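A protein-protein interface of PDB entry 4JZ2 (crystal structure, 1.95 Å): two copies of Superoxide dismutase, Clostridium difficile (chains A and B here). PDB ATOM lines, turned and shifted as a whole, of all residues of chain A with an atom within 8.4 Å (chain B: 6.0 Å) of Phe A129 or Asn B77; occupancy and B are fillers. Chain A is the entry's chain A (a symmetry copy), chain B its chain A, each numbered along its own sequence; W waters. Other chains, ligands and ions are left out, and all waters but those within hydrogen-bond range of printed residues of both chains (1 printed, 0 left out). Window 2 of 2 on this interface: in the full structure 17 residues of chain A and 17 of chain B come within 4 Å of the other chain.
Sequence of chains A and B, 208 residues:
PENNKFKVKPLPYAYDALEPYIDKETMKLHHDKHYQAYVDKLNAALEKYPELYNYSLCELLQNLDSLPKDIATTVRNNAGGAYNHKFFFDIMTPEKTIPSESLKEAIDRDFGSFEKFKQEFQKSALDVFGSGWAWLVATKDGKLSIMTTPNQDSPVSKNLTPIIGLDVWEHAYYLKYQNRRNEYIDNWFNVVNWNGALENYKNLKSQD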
ATOM      1  N   SER A 124      -9.517   1.387  24.781  1.00  0.00           N
ATOM      2  CA  SER A 124      -9.679  -0.061  24.812  1.00  0.00           C
ATOM      3  C   SER A 124     -11.143  -0.435  24.554  1.00  0.00           C
ATOM      4  O   SER A 124     -11.426  -1.363  23.792  1.00  0.00           O
ATOM      5  CB  SER A 124      -9.184  -0.646  26.140  1.00  0.00           C
ATOM      6  OG  SER A 124      -7.778  -0.433  26.290  1.00  0.00           O
ATOM      7  N   ALA A 125     -12.070   0.287  25.177  1.00  0.00           N
ATOM      8  CA  ALA A 125     -13.497   0.017  24.970  1.00  0.00           C
ATOM      9  C   ALA A 125     -13.894   0.222  23.505  1.00  0.00           C
ATOM     10  O   ALA A 125     -14.654  -0.564  22.930  1.00  0.00           O
ATOM     11  CB  ALA A 125     -14.341   0.907  25.867  1.00  0.00           C
ATOM     12  N   LEU A 126     -13.368   1.278  22.906  1.00  0.00           N
ATOM     13  CA  LEU A 126     -13.711   1.605  21.535  1.00  0.00           C
ATOM     14  C   LEU A 126     -13.170   0.528  20.597  1.00  0.00           C
ATOM     15  O   LEU A 126     -13.806   0.181  19.605  1.00  0.00           O
ATOM     16  CB  LEU A 126     -13.136   2.976  21.176  1.00  0.00           C
ATOM     17  CG  LEU A 126     -13.589   3.590  19.856  1.00  0.00           C
ATOM     18  CD1 LEU A 126     -15.040   4.011  19.953  1.00  0.00           C
ATOM     19  CD2 LEU A 126     -12.708   4.778  19.496  1.00  0.00           C
ATOM     20  N   ASP A 127     -12.008  -0.029  20.934  1.00  0.00           N
ATOM     21  CA  ASP A 127     -11.333  -0.956  20.029  1.00  0.00           C
ATOM     22  C   ASP A 127     -11.809  -2.417  20.100  1.00  0.00           C
ATOM     23  O   ASP A 127     -11.386  -3.247  19.291  1.00  0.00           O
ATOM     24  CB  ASP A 127      -9.809  -0.865  20.207  1.00  0.00           C
ATOM     25  CG  ASP A 127      -9.240   0.463  19.714  1.00  0.00           C
ATOM     26  OD1 ASP A 127      -9.981   1.229  19.054  1.00  0.00           O
ATOM     27  OD2 ASP A 127      -8.050   0.747  19.990  1.00  0.00           O
ATOM     28  N   VAL A 128     -12.684  -2.740  21.052  1.00  0.00           N
ATOM     29  CA  VAL A 128     -13.242  -4.081  21.109  1.00  0.00           C
ATOM     30  C   VAL A 128     -13.935  -4.354  19.779  1.00  0.00           C
ATOM     31  O   VAL A 128     -14.799  -3.587  19.366  1.00  0.00           O
ATOM     32  CB  VAL A 128     -14.255  -4.250  22.261  1.00  0.00           C
ATOM     33  CG1 VAL A 128     -14.946  -5.602  22.163  1.00  0.00           C
ATOM     34  CG2 VAL A 128     -13.549  -4.122  23.612  1.00  0.00           C
ATOM     35  N   PHE A 129     -13.524  -5.425  19.099  1.00  0.00           N
ATOM     36  CA  PHE A 129     -14.110  -5.768  17.806  1.00  0.00           C
ATOM     37  C   PHE A 129     -15.109  -6.895  17.985  1.00  0.00           C
ATOM     38  O   PHE A 129     -14.757  -7.982  18.455  1.00  0.00           O
ATOM     39  CB  PHE A 129     -13.040  -6.174  16.784  1.00  0.00           C
ATOM     40  CG  PHE A 129     -13.580  -6.324  15.386  1.00  0.00           C
ATOM     41  CD1 PHE A 129     -13.756  -5.209  14.575  1.00  0.00           C
ATOM     42  CD2 PHE A 129     -13.937  -7.569  14.893  1.00  0.00           C
ATOM     43  CE1 PHE A 129     -14.275  -5.334  13.293  1.00  0.00           C
ATOM     44  CE2 PHE A 129     -14.459  -7.696  13.604  1.00  0.00           C
ATOM     45  CZ  PHE A 129     -14.627  -6.579  12.812  1.00  0.00           C
ATOM     46  N   GLY A 130     -16.353  -6.642  17.602  1.00  0.00           N
ATOM     47  CA  GLY A 130     -17.431  -7.578  17.889  1.00  0.00           C
ATOM     48  C   GLY A 130     -17.995  -7.292  19.269  1.00  0.00           C
ATOM     49  O   GLY A 130     -17.932  -6.150  19.722  1.00  0.00           O
ATOM     50  N   SER A 131     -18.545  -8.316  19.933  1.00  0.00           N
ATOM     51  CA  SER A 131     -19.176  -8.158  21.246  1.00  0.00           C
ATOM     52  C   SER A 131     -18.120  -8.338  22.345  1.00  0.00           C
ATOM     53  O   SER A 131     -17.197  -9.129  22.190  1.00  0.00           O
ATOM     54  CB  SER A 131     -20.289  -9.196  21.435  1.00  0.00           C
ATOM     55  OG  SER A 131     -21.224  -9.160  20.354  1.00  0.00           O
ATOM     56  N   GLY A 132     -18.247  -7.607  23.451  1.00  0.00           N
ATOM     57  CA  GLY A 132     -17.321  -7.800  24.554  1.00  0.00           C
ATOM     58  C   GLY A 132     -17.365  -6.717  25.613  1.00  0.00           C
ATOM     59  O   GLY A 132     -18.330  -5.963  25.690  1.00  0.00           O
ATOM     60  N   TRP A 133     -16.293  -6.626  26.396  1.00  0.00           N
ATOM     61  CA  TRP A 133     -16.251  -5.789  27.592  1.00  0.00           C
ATOM     62  C   TRP A 133     -14.889  -5.141  27.720  1.00  0.00           C
ATOM     63  O   TRP A 133     -13.871  -5.713  27.302  1.00  0.00           O
ATOM     64  CB  TRP A 133     -16.471  -6.643  28.846  1.00  0.00           C
ATOM     65  CG  TRP A 133     -17.818  -7.254  28.937  1.00  0.00           C
ATOM     66  CD1 TRP A 133     -18.266  -8.355  28.264  1.00  0.00           C
ATOM     67  CD2 TRP A 133     -18.896  -6.828  29.772  1.00  0.00           C
ATOM     68  NE1 TRP A 133     -19.564  -8.632  28.617  1.00  0.00           N
ATOM     69  CE2 TRP A 133     -19.979  -7.699  29.540  1.00  0.00           C
ATOM     70  CE3 TRP A 133     -19.055  -5.784  30.693  1.00  0.00           C
ATOM     71  CZ2 TRP A 133     -21.204  -7.570  30.196  1.00  0.00           C
ATOM     72  CZ3 TRP A 133     -20.274  -5.649  31.340  1.00  0.00           C
ATOM     73  CH2 TRP A 133     -21.333  -6.540  31.089  1.00  0.00           C
ATOM     74  N   THR A 148      -9.543  -6.184  27.921  1.00  0.00           N
ATOM     75  CA  THR A 148     -10.865  -6.446  27.358  1.00  0.00           C
ATOM     76  C   THR A 148     -11.106  -7.941  27.301  1.00  0.00           C
ATOM     77  O   THR A 148     -10.155  -8.728  27.314  1.00  0.00           O
ATOM     78  CB  THR A 148     -10.984  -5.885  25.931  1.00  0.00           C
ATOM     79  OG1 THR A 148     -10.048  -6.564  25.079  1.00  0.00           O
ATOM     80  CG2 THR A 148     -10.679  -4.414  25.919  1.00  0.00           C
ATOM     81  N   THR A 149     -12.377  -8.336  27.251  1.00  0.00           N
ATOM     82  CA  THR A 149     -12.734  -9.729  27.035  1.00  0.00           C
ATOM     83  C   THR A 149     -13.778  -9.804  25.930  1.00  0.00           C
ATOM     84  O   THR A 149     -14.582  -8.874  25.764  1.00  0.00           O
ATOM     85  CB  THR A 149     -13.332 -10.386  28.287  1.00  0.00           C
ATOM     86  OG1 THR A 149     -14.462  -9.621  28.728  1.00  0.00           O
ATOM     87  CG2 THR A 149     -12.283 -10.489  29.410  1.00  0.00           C
ATOM     88  N   PRO A 150     -13.768 -10.910  25.168  1.00  0.00           N
ATOM     89  CA  PRO A 150     -14.764 -11.087  24.107  1.00  0.00           C
ATOM     90  C   PRO A 150     -16.055 -11.687  24.647  1.00  0.00           C
ATOM     91  O   PRO A 150     -16.023 -12.423  25.636  1.00  0.00           O
ATOM     92  CB  PRO A 150     -14.080 -12.099  23.177  1.00  0.00           C
ATOM     93  CG  PRO A 150     -13.310 -12.968  24.130  1.00  0.00           C
ATOM     94  CD  PRO A 150     -12.736 -11.965  25.130  1.00  0.00           C
ATOM     95  N   ASN A 151     -17.174 -11.423  23.974  1.00  0.00           N
ATOM     96  CA  ASN A 151     -18.441 -12.049  24.339  1.00  0.00           C
ATOM     97  C   ASN A 151     -18.737 -11.919  25.835  1.00  0.00           C
ATOM     98  O   ASN A 151     -18.794 -10.806  26.348  1.00  0.00           O
ATOM     99  CB  ASN A 151     -18.469 -13.495  23.821  1.00  0.00           C
ATOM    100  CG  ASN A 151     -18.145 -13.548  22.331  1.00  0.00           C
ATOM    101  OD1 ASN A 151     -18.578 -12.673  21.568  1.00  0.00           O
ATOM    102  ND2 ASN A 151     -17.335 -14.525  21.920  1.00  0.00           N
ATOM    103  N   VAL A 168     -19.760  -3.440  26.024  1.00  0.00           N
ATOM    104  CA  VAL A 168     -19.817  -2.834  24.682  1.00  0.00           C
ATOM    105  C   VAL A 168     -20.438  -3.737  23.621  1.00  0.00           C
ATOM    106  O   VAL A 168     -20.229  -3.537  22.416  1.00  0.00           O
ATOM    107  CB  VAL A 168     -18.466  -2.244  24.186  1.00  0.00           C
ATOM    108  CG1 VAL A 168     -18.048  -1.074  25.073  1.00  0.00           C
ATOM    109  CG2 VAL A 168     -17.386  -3.331  24.122  1.00  0.00           C
ATOM    110  N   ARG A 181     -20.445   4.284  19.282  1.00  0.00           N
ATOM    111  CA  ARG A 181     -20.030   3.694  20.547  1.00  0.00           C
ATOM    112  C   ARG A 181     -19.172   4.679  21.329  1.00  0.00           C
ATOM    113  O   ARG A 181     -19.235   4.725  22.561  1.00  0.00           O
ATOM    114  CB  ARG A 181     -19.270   2.377  20.332  1.00  0.00           C
ATOM    115  CG  ARG A 181     -19.023   1.596  21.636  1.00  0.00           C
ATOM    116  CD  ARG A 181     -17.899   0.553  21.466  1.00  0.00           C
ATOM    117  NE  ARG A 181     -18.282  -0.557  20.586  1.00  0.00           N
ATOM    118  CZ  ARG A 181     -17.449  -1.548  20.253  1.00  0.00           C
ATOM    119  NH1 ARG A 181     -16.198  -1.562  20.718  1.00  0.00           N
ATOM    120  NH2 ARG A 181     -17.854  -2.524  19.454  1.00  0.00           N
ATOM    121  N   TYR B  38     -15.994  -0.176   7.675  1.00  0.00           N
ATOM    122  CA  TYR B  38     -15.118  -1.290   7.328  1.00  0.00           C
ATOM    123  C   TYR B  38     -14.285  -0.939   6.106  1.00  0.00           C
ATOM    124  O   TYR B  38     -13.089  -1.208   6.063  1.00  0.00           O
ATOM    125  CB  TYR B  38     -15.918  -2.564   7.067  1.00  0.00           C
ATOM    126  CG  TYR B  38     -16.581  -3.119   8.311  1.00  0.00           C
ATOM    127  CD1 TYR B  38     -15.830  -3.451   9.434  1.00  0.00           C
ATOM    128  CD2 TYR B  38     -17.948  -3.311   8.359  1.00  0.00           C
ATOM    129  CE1 TYR B  38     -16.437  -3.962  10.578  1.00  0.00           C
ATOM    130  CE2 TYR B  38     -18.565  -3.810   9.495  1.00  0.00           C
ATOM    131  CZ  TYR B  38     -17.802  -4.131  10.602  1.00  0.00           C
ATOM    132  OH  TYR B  38     -18.433  -4.640  11.721  1.00  0.00           O
ATOM    133  N   ALA B  72      -2.429  -8.135   9.254  1.00  0.00           N
ATOM    134  CA  ALA B  72      -3.191  -9.355   9.055  1.00  0.00           C
ATOM    135  C   ALA B  72      -4.544  -9.289   9.764  1.00  0.00           C
ATOM    136  O   ALA B  72      -5.578  -9.648   9.194  1.00  0.00           O
ATOM    137  CB  ALA B  72      -2.400 -10.554   9.539  1.00  0.00           C
ATOM    138  N   THR B  73      -4.531  -8.846  11.018  1.00  0.00           N
ATOM    139  CA  THR B  73      -5.750  -8.830  11.824  1.00  0.00           C
ATOM    140  C   THR B  73      -6.704  -7.742  11.352  1.00  0.00           C
ATOM    141  O   THR B  73      -7.905  -7.973  11.218  1.00  0.00           O
ATOM    142  CB  THR B  73      -5.427  -8.647  13.319  1.00  0.00           C
ATOM    143  OG1 THR B  73      -4.793  -9.839  13.793  1.00  0.00           O
ATOM    144  CG2 THR B  73      -6.697  -8.408  14.118  1.00  0.00           C
ATOM    145  N   THR B  74      -6.166  -6.563  11.076  1.00  0.00           N
ATOM    146  CA  THR B  74      -7.017  -5.467  10.636  1.00  0.00           C
ATOM    147  C   THR B  74      -7.679  -5.809   9.295  1.00  0.00           C
ATOM    148  O   THR B  74      -8.841  -5.480   9.067  1.00  0.00           O
ATOM    149  CB  THR B  74      -6.256  -4.132  10.579  1.00  0.00           C
ATOM    150  OG1 THR B  74      -7.125  -3.105  10.086  1.00  0.00           O
ATOM    151  CG2 THR B  74      -5.061  -4.241   9.668  1.00  0.00           C
ATOM    152  N   VAL B  75      -6.944  -6.487   8.416  1.00  0.00           N
ATOM    153  CA  VAL B  75      -7.490  -6.861   7.118  1.00  0.00           C
ATOM    154  C   VAL B  75      -8.551  -7.938   7.297  1.00  0.00           C
ATOM    155  O   VAL B  75      -9.617  -7.896   6.684  1.00  0.00           O
ATOM    156  CB  VAL B  75      -6.380  -7.327   6.148  1.00  0.00           C
ATOM    157  CG1 VAL B  75      -6.987  -8.035   4.930  1.00  0.00           C
ATOM    158  CG2 VAL B  75      -5.524  -6.133   5.729  1.00  0.00           C
ATOM    159  N   ARG B  76      -8.266  -8.904   8.159  1.00  0.00           N
ATOM    160  CA  ARG B  76      -9.241  -9.944   8.465  1.00  0.00           C
ATOM    161  C   ARG B  76     -10.569  -9.309   8.907  1.00  0.00           C
ATOM    162  O   ARG B  76     -11.629  -9.634   8.385  1.00  0.00           O
ATOM    163  CB  ARG B  76      -8.700 -10.863   9.560  1.00  0.00           C
ATOM    164  CG  ARG B  76      -9.696 -11.860  10.133  1.00  0.00           C
ATOM    165  CD  ARG B  76      -9.034 -12.632  11.278  1.00  0.00           C
ATOM    166  NE  ARG B  76      -9.941 -13.564  11.932  1.00  0.00           N
ATOM    167  CZ  ARG B  76      -9.589 -14.369  12.935  1.00  0.00           C
ATOM    168  NH1 ARG B  76      -8.340 -14.350  13.396  1.00  0.00           N
ATOM    169  NH2 ARG B  76     -10.475 -15.199  13.478  1.00  0.00           N
ATOM    170  N   ASN B  77     -10.504  -8.390   9.864  1.00  0.00           N
ATOM    171  CA  ASN B  77     -11.728  -7.764  10.380  1.00  0.00           C
ATOM    172  C   ASN B  77     -12.417  -6.850   9.364  1.00  0.00           C
ATOM    173  O   ASN B  77     -13.636  -6.890   9.195  1.00  0.00           O
ATOM    174  CB  ASN B  77     -11.421  -6.991  11.657  1.00  0.00           C
ATOM    175  CG  ASN B  77     -11.019  -7.904  12.807  1.00  0.00           C
ATOM    176  OD1 ASN B  77     -11.327  -9.100  12.806  1.00  0.00           O
ATOM    177  ND2 ASN B  77     -10.321  -7.343  13.794  1.00  0.00           N
ATOM    178  N   ASN B  78     -11.634  -6.027   8.686  1.00  0.00           N
ATOM    179  CA  ASN B  78     -12.217  -5.008   7.823  1.00  0.00           C
ATOM    180  C   ASN B  78     -12.479  -5.445   6.380  1.00  0.00           C
ATOM    181  O   ASN B  78     -13.475  -5.036   5.790  1.00  0.00           O
ATOM    182  CB  ASN B  78     -11.406  -3.727   7.902  1.00  0.00           C
ATOM    183  CG  ASN B  78     -11.439  -3.126   9.294  1.00  0.00           C
ATOM    184  OD1 ASN B  78     -10.444  -3.152  10.024  1.00  0.00           O
ATOM    185  ND2 ASN B  78     -12.604  -2.630   9.688  1.00  0.00           N
ATOM    186  N   ALA B  79     -11.615  -6.284   5.809  1.00  0.00           N
ATOM    187  CA  ALA B  79     -11.941  -6.868   4.511  1.00  0.00           C
ATOM    188  C   ALA B  79     -13.129  -7.790   4.724  1.00  0.00           C
ATOM    189  O   ALA B  79     -14.021  -7.879   3.885  1.00  0.00           O
ATOM    190  CB  ALA B  79     -10.741  -7.651   3.919  1.00  0.00           C
ATOM    191  N   GLY B  80     -13.134  -8.474   5.863  1.00  0.00           N
ATOM    192  CA  GLY B  80     -14.254  -9.313   6.228  1.00  0.00           C
ATOM    193  C   GLY B  80     -15.535  -8.494   6.252  1.00  0.00           C
ATOM    194  O   GLY B  80     -16.526  -8.857   5.616  1.00  0.00           O
ATOM    195  N   GLY B  81     -15.504  -7.380   6.976  1.00  0.00           N
ATOM    196  CA  GLY B  81     -16.670  -6.517   7.094  1.00  0.00           C
ATOM    197  C   GLY B  81     -17.127  -5.985   5.745  1.00  0.00           C
ATOM    198  O   GLY B  81     -18.320  -5.963   5.438  1.00  0.00           O
ATOM    199  N   ALA B  82     -16.170  -5.543   4.941  1.00  0.00           N
ATOM    200  CA  ALA B  82     -16.472  -4.989   3.627  1.00  0.00           C
ATOM    201  C   ALA B  82     -17.089  -6.059   2.733  1.00  0.00           C
ATOM    202  O   ALA B  82     -18.111  -5.830   2.084  1.00  0.00           O
ATOM    203  CB  ALA B  82     -15.218  -4.416   2.988  1.00  0.00           C
ATOM    204  N   ASN B 151     -17.826 -12.638  14.466  1.00  0.00           N
ATOM    205  CA  ASN B 151     -17.400 -11.300  14.068  1.00  0.00           C
ATOM    206  C   ASN B 151     -17.508 -11.089  12.556  1.00  0.00           C
ATOM    207  O   ASN B 151     -18.590 -11.237  11.999  1.00  0.00           O
ATOM    208  CB  ASN B 151     -16.004 -11.014  14.640  1.00  0.00           C
ATOM    209  CG  ASN B 151     -15.967 -11.266  16.144  1.00  0.00           C
ATOM    210  OD1 ASN B 151     -16.936 -10.954  16.853  1.00  0.00           O
ATOM    211  ND2 ASN B 151     -14.891 -11.885  16.631  1.00  0.00           N
ATOM    212  N   GLN B 152     -16.420 -10.734  11.891  1.00  0.00           N
ATOM    213  CA  GLN B 152     -16.476 -10.578  10.433  1.00  0.00           C
ATOM    214  C   GLN B 152     -15.683 -11.661   9.706  1.00  0.00           C
ATOM    215  O   GLN B 152     -15.274 -11.478   8.550  1.00  0.00           O
ATOM    216  CB  GLN B 152     -15.993  -9.191   9.993  1.00  0.00           C
ATOM    217  CG  GLN B 152     -16.881  -8.014  10.491  1.00  0.00           C
ATOM    218  CD  GLN B 152     -18.342  -8.126  10.060  1.00  0.00           C
ATOM    219  OE1 GLN B 152     -18.688  -8.905   9.167  1.00  0.00           O
ATOM    220  NE2 GLN B 152     -19.211  -7.337  10.699  1.00  0.00           N
ATOM    221  N   ASP B 153     -15.460 -12.790  10.368  1.00  0.00           N
ATOM    222  CA  ASP B 153     -14.799 -13.894   9.678  1.00  0.00           C
ATOM    223  C   ASP B 153     -15.714 -14.370   8.544  1.00  0.00           C
ATOM    224  O   ASP B 153     -16.930 -14.186   8.607  1.00  0.00           O
ATOM    225  CB  ASP B 153     -14.427 -15.010  10.649  1.00  0.00           C
ATOM    226  CG  ASP B 153     -13.328 -14.578  11.632  1.00  0.00           C
ATOM    227  OD1 ASP B 153     -12.721 -13.508  11.422  1.00  0.00           O
ATOM    228  OD2 ASP B 153     -13.068 -15.305  12.609  1.00  0.00           O
ATOM    229  N   TRP B 169     -25.081  -9.781  13.925  1.00  0.00           N
ATOM    230  CA  TRP B 169     -24.611  -8.714  14.800  1.00  0.00           C
ATOM    231  C   TRP B 169     -25.874  -7.998  15.272  1.00  0.00           C
ATOM    232  O   TRP B 169     -26.829  -7.850  14.501  1.00  0.00           O
ATOM    233  CB  TRP B 169     -23.754  -7.734  14.020  1.00  0.00           C
ATOM    234  CG  TRP B 169     -22.329  -8.202  13.768  1.00  0.00           C
ATOM    235  CD1 TRP B 169     -21.933  -9.349  13.124  1.00  0.00           C
ATOM    236  CD2 TRP B 169     -21.131  -7.526  14.154  1.00  0.00           C
ATOM    237  NE1 TRP B 169     -20.550  -9.419  13.083  1.00  0.00           N
ATOM    238  CE2 TRP B 169     -20.037  -8.302  13.713  1.00  0.00           C
ATOM    239  CE3 TRP B 169     -20.869  -6.321  14.830  1.00  0.00           C
ATOM    240  CZ2 TRP B 169     -18.712  -7.927  13.927  1.00  0.00           C
ATOM    241  CZ3 TRP B 169     -19.550  -5.944  15.042  1.00  0.00           C
ATOM    242  CH2 TRP B 169     -18.485  -6.747  14.593  1.00  0.00           C
HETATM  243  O   HOH W   1     -18.563 -11.131  19.178  1.00  0.00           O
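The side-chain hydroxyl (OH) of Tyr B38 sits at hydrogen-bond distance from the side-chain amide nitrogen (NE2) of Gln B152 (3.0 Å). NE1 of Trp B169 lies within hydrogen-bond range of O of Asn B151, at 2.9 Å. NE1 of Trp B169 sits close to NE2 of Gln B152, 3.4 Å away.
Among the printed residues, pairs that only touch across the chains: Phe A129 with Asn B77, Phe A129 with Gln B152, Gly A130 with Trp B169, Gly A130 with Asn B151, Phe A129 with Tyr B38 and Phe A129 with Asn B151.
Printed residues of chain B within 4 Å of Phe A129: Tyr B38, Asn B77, Asn B151 and Gln B152. Gly A132 touches none of the printed residues of chain B. Of the printed residues of chain A, Tyr B38 touches Phe A129. Asn B77 touches just one residue of chain A: Phe A129. No residue of chain A comes within 4 Å of Asn B78. Ala B82 touches none of the printed residues of chain A. Of the printed residues of chain A, Asn B151 touches Phe A129 (3.8 Å) and Gly A130 (3.6 Å). Printed residues of chain A within 4 Å of Trp B169: Gly A130.
Hydrophobic or aromatic side chains of chain A within 4 Å of the printed part of chain B: Phe A129. Among the printed residues, 6 pairs touch across the chains. Among the printed residues, no Asp or Glu carboxylate lies within 4 Å of a Lys or Arg side-chain nitrogen of the other chain.
Position printed for both chains: 151. Of the 6 pairs that touch across the chains among the printed residues, none has its exchanged pair printed and touching as well.
Water W1 lies within hydrogen-bond range of the side-chain amide oxygen of Asn A151 (2.8 Å), the side-chain amide oxygen of Asn B151 (2.8 Å) and the backbone NH of Ser A131 (2.9 Å).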
